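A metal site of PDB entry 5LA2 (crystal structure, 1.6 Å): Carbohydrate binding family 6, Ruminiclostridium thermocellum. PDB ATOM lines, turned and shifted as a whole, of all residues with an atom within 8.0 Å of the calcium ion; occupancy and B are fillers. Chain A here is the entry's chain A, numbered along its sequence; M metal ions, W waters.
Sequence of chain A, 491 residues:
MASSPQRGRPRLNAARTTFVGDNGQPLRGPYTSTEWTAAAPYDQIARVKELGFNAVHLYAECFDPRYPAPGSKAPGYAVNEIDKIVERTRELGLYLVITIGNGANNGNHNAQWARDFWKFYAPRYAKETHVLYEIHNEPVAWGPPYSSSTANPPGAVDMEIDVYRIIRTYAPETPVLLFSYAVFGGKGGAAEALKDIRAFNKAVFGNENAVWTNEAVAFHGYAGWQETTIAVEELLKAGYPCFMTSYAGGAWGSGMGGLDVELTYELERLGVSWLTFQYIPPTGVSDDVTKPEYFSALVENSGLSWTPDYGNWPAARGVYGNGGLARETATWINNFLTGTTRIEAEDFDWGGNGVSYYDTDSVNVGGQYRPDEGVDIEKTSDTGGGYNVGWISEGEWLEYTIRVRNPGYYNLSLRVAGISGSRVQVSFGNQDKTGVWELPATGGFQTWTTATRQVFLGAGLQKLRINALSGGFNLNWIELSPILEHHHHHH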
ATOM      1  N   ARG A 342      -3.523 -14.346 -23.735  1.00  0.00           N
ATOM      2  CA  ARG A 342      -2.947 -15.684 -23.877  1.00  0.00           C
ATOM      3  C   ARG A 342      -1.571 -15.587 -24.524  1.00  0.00           C
ATOM      4  O   ARG A 342      -1.341 -14.855 -25.518  1.00  0.00           O
ATOM      5  CB  ARG A 342      -3.850 -16.656 -24.660  1.00  0.00           C
ATOM      6  CG  ARG A 342      -3.349 -18.103 -24.623  1.00  0.00           C
ATOM      7  CD  ARG A 342      -4.322 -19.132 -25.195  1.00  0.00           C
ATOM      8  NE  ARG A 342      -5.433 -19.418 -24.293  1.00  0.00           N
ATOM      9  CZ  ARG A 342      -6.321 -20.397 -24.475  1.00  0.00           C
ATOM     10  NH1 ARG A 342      -6.246 -21.224 -25.516  1.00  0.00           N
ATOM     11  NH2 ARG A 342      -7.294 -20.551 -23.581  1.00  0.00           N
ATOM     12  N   ILE A 343      -0.644 -16.326 -23.913  1.00  0.00           N
ATOM     13  CA  ILE A 343       0.702 -16.515 -24.451  1.00  0.00           C
ATOM     14  C   ILE A 343       0.909 -18.005 -24.603  1.00  0.00           C
ATOM     15  O   ILE A 343       0.897 -18.757 -23.618  1.00  0.00           O
ATOM     16  CB  ILE A 343       1.770 -15.877 -23.577  1.00  0.00           C
ATOM     17  CG1 ILE A 343       1.454 -14.396 -23.287  1.00  0.00           C
ATOM     18  CG2 ILE A 343       3.149 -16.044 -24.206  1.00  0.00           C
ATOM     19  CD1 ILE A 343       1.185 -14.169 -21.836  1.00  0.00           C
ATOM     20  N   GLU A 344       1.096 -18.446 -25.849  1.00  0.00           N
ATOM     21  CA  GLU A 344       1.323 -19.871 -26.092  1.00  0.00           C
ATOM     22  C   GLU A 344       2.711 -20.254 -25.607  1.00  0.00           C
ATOM     23  O   GLU A 344       3.648 -19.515 -25.787  1.00  0.00           O
ATOM     24  CB  GLU A 344       1.149 -20.172 -27.565  1.00  0.00           C
ATOM     25  CG  GLU A 344      -0.301 -19.956 -28.094  1.00  0.00           C
ATOM     26  CD  GLU A 344      -1.324 -20.893 -27.458  1.00  0.00           C
ATOM     27  OE1 GLU A 344      -0.935 -21.937 -26.969  1.00  0.00           O
ATOM     28  OE2 GLU A 344      -2.532 -20.562 -27.446  1.00  0.00           O
ATOM     29  N   ALA A 345       2.831 -21.414 -24.980  1.00  0.00           N
ATOM     30  CA  ALA A 345       4.115 -21.818 -24.391  1.00  0.00           C
ATOM     31  C   ALA A 345       5.171 -21.938 -25.496  1.00  0.00           C
ATOM     32  O   ALA A 345       6.360 -21.650 -25.267  1.00  0.00           O
ATOM     33  CB  ALA A 345       3.979 -23.125 -23.642  1.00  0.00           C
ATOM     34  N   GLU A 346       4.713 -22.330 -26.691  1.00  0.00           N
ATOM     35  CA  GLU A 346       5.566 -22.531 -27.845  1.00  0.00           C
ATOM     36  C   GLU A 346       6.020 -21.226 -28.525  1.00  0.00           C
ATOM     37  O   GLU A 346       6.824 -21.291 -29.444  1.00  0.00           O
ATOM     38  CB  GLU A 346       4.921 -23.463 -28.890  1.00  0.00           C
ATOM     39  CG  GLU A 346       3.595 -22.980 -29.527  1.00  0.00           C
ATOM     40  CD  GLU A 346       2.344 -23.369 -28.737  1.00  0.00           C
ATOM     41  OE1 GLU A 346       2.399 -23.532 -27.496  1.00  0.00           O
ATOM     42  OE2 GLU A 346       1.267 -23.501 -29.340  1.00  0.00           O
ATOM     43  N   ASP A 347       5.548 -20.057 -28.042  1.00  0.00           N
ATOM     44  CA  ASP A 347       5.916 -18.741 -28.597  1.00  0.00           C
ATOM     45  C   ASP A 347       6.873 -18.014 -27.706  1.00  0.00           C
ATOM     46  O   ASP A 347       6.847 -16.800 -27.634  1.00  0.00           O
ATOM     47  CB  ASP A 347       4.648 -17.887 -28.844  1.00  0.00           C
ATOM     48  CG  ASP A 347       3.812 -18.388 -30.020  1.00  0.00           C
ATOM     49  OD1 ASP A 347       4.348 -19.190 -30.811  1.00  0.00           O
ATOM     50  OD2 ASP A 347       2.645 -17.947 -30.151  1.00  0.00           O
ATOM     51  N   TYR A 369       6.774 -27.250 -34.919  1.00  0.00           N
ATOM     52  CA  TYR A 369       6.585 -25.799 -34.817  1.00  0.00           C
ATOM     53  C   TYR A 369       7.855 -24.984 -34.984  1.00  0.00           C
ATOM     54  O   TYR A 369       7.915 -24.127 -35.856  1.00  0.00           O
ATOM     55  CB  TYR A 369       5.900 -25.444 -33.493  1.00  0.00           C
ATOM     56  CG  TYR A 369       5.350 -24.042 -33.426  1.00  0.00           C
ATOM     57  CD1 TYR A 369       4.303 -23.635 -34.263  1.00  0.00           C
ATOM     58  CD2 TYR A 369       5.816 -23.141 -32.474  1.00  0.00           C
ATOM     59  CE1 TYR A 369       3.789 -22.350 -34.182  1.00  0.00           C
ATOM     60  CE2 TYR A 369       5.300 -21.878 -32.383  1.00  0.00           C
ATOM     61  CZ  TYR A 369       4.284 -21.477 -33.219  1.00  0.00           C
ATOM     62  OH  TYR A 369       3.807 -20.230 -33.089  1.00  0.00           O
ATOM     63  N   ILE A 377       8.820 -29.517 -28.517  1.00  0.00           N
ATOM     64  CA  ILE A 377       7.492 -29.135 -28.895  1.00  0.00           C
ATOM     65  C   ILE A 377       6.786 -30.235 -29.699  1.00  0.00           C
ATOM     66  O   ILE A 377       7.343 -30.726 -30.685  1.00  0.00           O
ATOM     67  CB  ILE A 377       7.463 -27.826 -29.702  1.00  0.00           C
ATOM     68  CG1 ILE A 377       8.250 -26.711 -29.005  1.00  0.00           C
ATOM     69  CG2 ILE A 377       6.030 -27.337 -29.846  1.00  0.00           C
ATOM     70  CD1 ILE A 377       8.440 -25.470 -29.859  1.00  0.00           C
ATOM     71  N   GLU A 378       5.561 -30.522 -29.295  1.00  0.00           N
ATOM     72  CA  GLU A 378       4.681 -31.539 -29.900  1.00  0.00           C
ATOM     73  C   GLU A 378       3.276 -30.957 -30.166  1.00  0.00           C
ATOM     74  O   GLU A 378       2.847 -29.959 -29.536  1.00  0.00           O
ATOM     75  CB  GLU A 378       4.567 -32.765 -28.974  1.00  0.00           C
ATOM     76  CG  GLU A 378       4.012 -32.451 -27.573  1.00  0.00           C
ATOM     77  CD  GLU A 378       4.009 -33.649 -26.640  1.00  0.00           C
ATOM     78  OE1 GLU A 378       4.064 -34.779 -27.139  1.00  0.00           O
ATOM     79  OE2 GLU A 378       3.941 -33.455 -25.404  1.00  0.00           O
ATOM     80  N   THR A 380      -0.625 -30.881 -29.598  1.00  0.00           N
ATOM     81  CA  THR A 380      -1.401 -31.185 -28.388  1.00  0.00           C
ATOM     82  C   THR A 380      -2.802 -31.569 -28.782  1.00  0.00           C
ATOM     83  O   THR A 380      -3.317 -31.070 -29.770  1.00  0.00           O
ATOM     84  CB  THR A 380      -1.463 -30.001 -27.395  1.00  0.00           C
ATOM     85  OG1 THR A 380      -2.119 -30.437 -26.215  1.00  0.00           O
ATOM     86  CG2 THR A 380      -2.208 -28.792 -27.958  1.00  0.00           C
ATOM     87  N   ASP A 382      -5.120 -30.971 -26.515  1.00  0.00           N
ATOM     88  CA  ASP A 382      -5.905 -30.088 -25.670  1.00  0.00           C
ATOM     89  C   ASP A 382      -6.908 -29.282 -26.517  1.00  0.00           C
ATOM     90  O   ASP A 382      -6.699 -29.088 -27.727  1.00  0.00           O
ATOM     91  CB  ASP A 382      -5.020 -29.107 -24.892  1.00  0.00           C
ATOM     92  CG  ASP A 382      -5.715 -28.510 -23.680  1.00  0.00           C
ATOM     93  OD1 ASP A 382      -6.798 -28.976 -23.260  1.00  0.00           O
ATOM     94  OD2 ASP A 382      -5.160 -27.528 -23.134  1.00  0.00           O
ATOM     95  N   THR A 383      -7.935 -28.783 -25.861  1.00  0.00           N
ATOM     96  CA  THR A 383      -8.908 -27.861 -26.468  1.00  0.00           C
ATOM     97  C   THR A 383      -8.172 -26.680 -27.145  1.00  0.00           C
ATOM     98  O   THR A 383      -7.307 -26.052 -26.532  1.00  0.00           O
ATOM     99  CB  THR A 383      -9.898 -27.314 -25.408  1.00  0.00           C
ATOM    100  OG1 THR A 383     -10.435 -28.418 -24.675  1.00  0.00           O
ATOM    101  CG2 THR A 383     -11.059 -26.579 -26.040  1.00  0.00           C
ATOM    102  N   GLY A 384      -8.521 -26.425 -28.395  1.00  0.00           N
ATOM    103  CA  GLY A 384      -7.889 -25.412 -29.213  1.00  0.00           C
ATOM    104  C   GLY A 384      -6.770 -25.957 -30.078  1.00  0.00           C
ATOM    105  O   GLY A 384      -6.296 -25.246 -30.966  1.00  0.00           O
ATOM    106  N   GLY A 385      -6.321 -27.174 -29.847  1.00  0.00           N
ATOM    107  CA  GLY A 385      -5.246 -27.760 -30.657  1.00  0.00           C
ATOM    108  C   GLY A 385      -3.946 -26.983 -30.581  1.00  0.00           C
ATOM    109  O   GLY A 385      -3.614 -26.384 -29.540  1.00  0.00           O
ATOM    110  N   GLY A 386      -3.230 -26.960 -31.696  1.00  0.00           N
ATOM    111  CA  GLY A 386      -1.913 -26.348 -31.742  1.00  0.00           C
ATOM    112  C   GLY A 386      -0.858 -27.206 -31.088  1.00  0.00           C
ATOM    113  O   GLY A 386      -0.814 -28.402 -31.362  1.00  0.00           O
ATOM    114  N   TYR A 387      -0.033 -26.629 -30.201  1.00  0.00           N
ATOM    115  CA  TYR A 387       1.168 -27.277 -29.702  1.00  0.00           C
ATOM    116  C   TYR A 387       1.337 -27.143 -28.195  1.00  0.00           C
ATOM    117  O   TYR A 387       0.810 -26.234 -27.597  1.00  0.00           O
ATOM    118  CB  TYR A 387       2.387 -26.732 -30.415  1.00  0.00           C
ATOM    119  CG  TYR A 387       2.285 -26.818 -31.928  1.00  0.00           C
ATOM    120  CD1 TYR A 387       2.633 -27.966 -32.587  1.00  0.00           C
ATOM    121  CD2 TYR A 387       1.792 -25.757 -32.667  1.00  0.00           C
ATOM    122  CE1 TYR A 387       2.531 -28.064 -33.952  1.00  0.00           C
ATOM    123  CE2 TYR A 387       1.674 -25.856 -34.057  1.00  0.00           C
ATOM    124  CZ  TYR A 387       2.037 -27.026 -34.681  1.00  0.00           C
ATOM    125  OH  TYR A 387       1.954 -27.156 -36.045  1.00  0.00           O
ATOM    126  N   ASN A 388       2.076 -28.054 -27.582  1.00  0.00           N
ATOM    127  CA  ASN A 388       2.501 -27.860 -26.209  1.00  0.00           C
ATOM    128  C   ASN A 388       4.011 -28.091 -26.139  1.00  0.00           C
ATOM    129  O   ASN A 388       4.585 -28.787 -26.979  1.00  0.00           O
ATOM    130  CB  ASN A 388       1.746 -28.720 -25.189  1.00  0.00           C
ATOM    131  CG  ASN A 388       1.991 -30.228 -25.345  1.00  0.00           C
ATOM    132  OD1 ASN A 388       1.268 -30.908 -26.067  1.00  0.00           O
ATOM    133  ND2 ASN A 388       3.011 -30.759 -24.652  1.00  0.00           N
ATOM    134  N   VAL A 389       4.631 -27.421 -25.176  1.00  0.00           N
ATOM    135  CA  VAL A 389       5.958 -27.725 -24.794  1.00  0.00           C
ATOM    136  C   VAL A 389       5.914 -28.976 -23.915  1.00  0.00           C
ATOM    137  O   VAL A 389       5.091 -29.089 -23.008  1.00  0.00           O
ATOM    138  CB  VAL A 389       6.605 -26.546 -24.018  1.00  0.00           C
ATOM    139  CG1 VAL A 389       7.987 -26.964 -23.523  1.00  0.00           C
ATOM    140  CG2 VAL A 389       6.683 -25.310 -24.918  1.00  0.00           C
ATOM    141  N   ARG A 415      -1.558 -23.752 -18.278  1.00  0.00           N
ATOM    142  CA  ARG A 415      -2.333 -24.883 -18.795  1.00  0.00           C
ATOM    143  C   ARG A 415      -1.348 -26.022 -18.880  1.00  0.00           C
ATOM    144  O   ARG A 415      -0.485 -26.004 -19.752  1.00  0.00           O
ATOM    145  CB  ARG A 415      -2.953 -24.532 -20.137  1.00  0.00           C
ATOM    146  CG  ARG A 415      -3.854 -25.609 -20.718  1.00  0.00           C
ATOM    147  CD  ARG A 415      -5.102 -25.835 -19.882  1.00  0.00           C
ATOM    148  NE  ARG A 415      -6.015 -26.792 -20.516  1.00  0.00           N
ATOM    149  CZ  ARG A 415      -7.173 -27.191 -20.003  1.00  0.00           C
ATOM    150  NH1 ARG A 415      -7.595 -26.747 -18.801  1.00  0.00           N
ATOM    151  NH2 ARG A 415      -7.915 -28.062 -20.677  1.00  0.00           N
ATOM    152  N   TRP A 448      -5.293 -32.407 -19.375  1.00  0.00           N
ATOM    153  CA  TRP A 448      -4.918 -31.002 -19.101  1.00  0.00           C
ATOM    154  C   TRP A 448      -5.787 -30.363 -18.048  1.00  0.00           C
ATOM    155  O   TRP A 448      -6.975 -30.697 -17.944  1.00  0.00           O
ATOM    156  CB  TRP A 448      -5.029 -30.195 -20.375  1.00  0.00           C
ATOM    157  CG  TRP A 448      -4.099 -30.638 -21.417  1.00  0.00           C
ATOM    158  CD1 TRP A 448      -4.333 -31.543 -22.442  1.00  0.00           C
ATOM    159  CD2 TRP A 448      -2.745 -30.216 -21.576  1.00  0.00           C
ATOM    160  NE1 TRP A 448      -3.201 -31.674 -23.223  1.00  0.00           N
ATOM    161  CE2 TRP A 448      -2.219 -30.867 -22.709  1.00  0.00           C
ATOM    162  CE3 TRP A 448      -1.927 -29.347 -20.857  1.00  0.00           C
ATOM    163  CZ2 TRP A 448      -0.880 -30.686 -23.127  1.00  0.00           C
ATOM    164  CZ3 TRP A 448      -0.605 -29.158 -21.279  1.00  0.00           C
ATOM    165  CH2 TRP A 448      -0.113 -29.801 -22.399  1.00  0.00           C
ATOM    166  N   LEU A 475       3.375 -27.988 -20.817  1.00  0.00           N
ATOM    167  CA  LEU A 475       2.830 -26.642 -20.735  1.00  0.00           C
ATOM    168  C   LEU A 475       2.261 -26.245 -22.109  1.00  0.00           C
ATOM    169  O   LEU A 475       2.987 -26.239 -23.119  1.00  0.00           O
ATOM    170  CB  LEU A 475       3.893 -25.650 -20.306  1.00  0.00           C
ATOM    171  CG  LEU A 475       3.468 -24.185 -20.140  1.00  0.00           C
ATOM    172  CD1 LEU A 475       2.513 -23.962 -18.989  1.00  0.00           C
ATOM    173  CD2 LEU A 475       4.696 -23.296 -19.947  1.00  0.00           C
ATOM    174  N   ASN A 476       0.965 -25.938 -22.142  1.00  0.00           N
ATOM    175  CA  ASN A 476       0.298 -25.595 -23.407  1.00  0.00           C
ATOM    176  C   ASN A 476       0.352 -24.069 -23.662  1.00  0.00           C
ATOM    177  O   ASN A 476       0.695 -23.584 -24.769  1.00  0.00           O
ATOM    178  CB  ASN A 476      -1.155 -26.069 -23.379  1.00  0.00           C
ATOM    179  CG  ASN A 476      -1.870 -25.854 -24.718  1.00  0.00           C
ATOM    180  OD1 ASN A 476      -1.309 -25.355 -25.692  1.00  0.00           O
ATOM    181  ND2 ASN A 476      -3.115 -26.252 -24.756  1.00  0.00           N
ATOM    182  N   TRP A 477      -0.023 -23.341 -22.630  1.00  0.00           N
ATOM    183  CA  TRP A 477      -0.113 -21.884 -22.674  1.00  0.00           C
ATOM    184  C   TRP A 477      -0.140 -21.294 -21.280  1.00  0.00           C
ATOM    185  O   TRP A 477      -0.255 -22.015 -20.277  1.00  0.00           O
ATOM    186  CB  TRP A 477      -1.321 -21.413 -23.518  1.00  0.00           C
ATOM    187  CG  TRP A 477      -2.684 -21.989 -23.202  1.00  0.00           C
ATOM    188  CD1 TRP A 477      -3.360 -22.876 -23.976  1.00  0.00           C
ATOM    189  CD2 TRP A 477      -3.533 -21.735 -22.062  1.00  0.00           C
ATOM    190  NE1 TRP A 477      -4.575 -23.156 -23.432  1.00  0.00           N
ATOM    191  CE2 TRP A 477      -4.702 -22.489 -22.252  1.00  0.00           C
ATOM    192  CE3 TRP A 477      -3.407 -20.949 -20.914  1.00  0.00           C
ATOM    193  CZ2 TRP A 477      -5.737 -22.483 -21.325  1.00  0.00           C
ATOM    194  CZ3 TRP A 477      -4.442 -20.943 -19.987  1.00  0.00           C
ATOM    195  CH2 TRP A 477      -5.596 -21.703 -20.202  1.00  0.00           C
ATOM    196  N   ILE A 478      -0.053 -19.969 -21.278  1.00  0.00           N
ATOM    197  CA  ILE A 478       0.006 -19.098 -20.118  1.00  0.00           C
ATOM    198  C   ILE A 478      -1.086 -18.051 -20.329  1.00  0.00           C
ATOM    199  O   ILE A 478      -1.240 -17.554 -21.451  1.00  0.00           O
ATOM    200  CB  ILE A 478       1.380 -18.370 -20.063  1.00  0.00           C
ATOM    201  CG1 ILE A 478       2.539 -19.375 -20.033  1.00  0.00           C
ATOM    202  CG2 ILE A 478       1.466 -17.425 -18.842  1.00  0.00           C
ATOM    203  CD1 ILE A 478       3.842 -18.842 -20.617  1.00  0.00           C
HETATM  204 CA    CA M   1       0.059 -24.126 -27.048  1.00  0.00          CA
HETATM  205  O   HOH W   1      -1.732 -24.379 -28.832  1.00  0.00           O
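The backbone carbonyl oxygen (O) of Arg 415 is in hydrogen-bond range of the backbone NH (N) of Asn 476 (2.8 Å). The backbone NH (N) of Ala 345 sits close to the backbone carbonyl oxygen (O) of Asn 476 (3.1 Å). The side-chain amide nitrogen (ND2) of Asn 476 sits at hydrogen-bond distance from the side-chain carboxylate (OD2) of Asp 382.
The calcium ion is bound by OD1 of Asn 476 (2.3 Å). The backbone carbonyl oxygen (O) of Tyr 387 is bound to the calcium ion (2.3 Å). OE1 of Glu 344 binds the calcium ion, 2.4 Å away. The calcium ion is bound by O of Asn 476 (2.4 Å). OE1 of Glu 346 is bound to the calcium ion (2.5 Å). Water W1 is bound to the calcium ion (2.5 Å). The side-chain carboxylate (OE2) of Glu 346 binds the calcium ion (2.7 Å).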
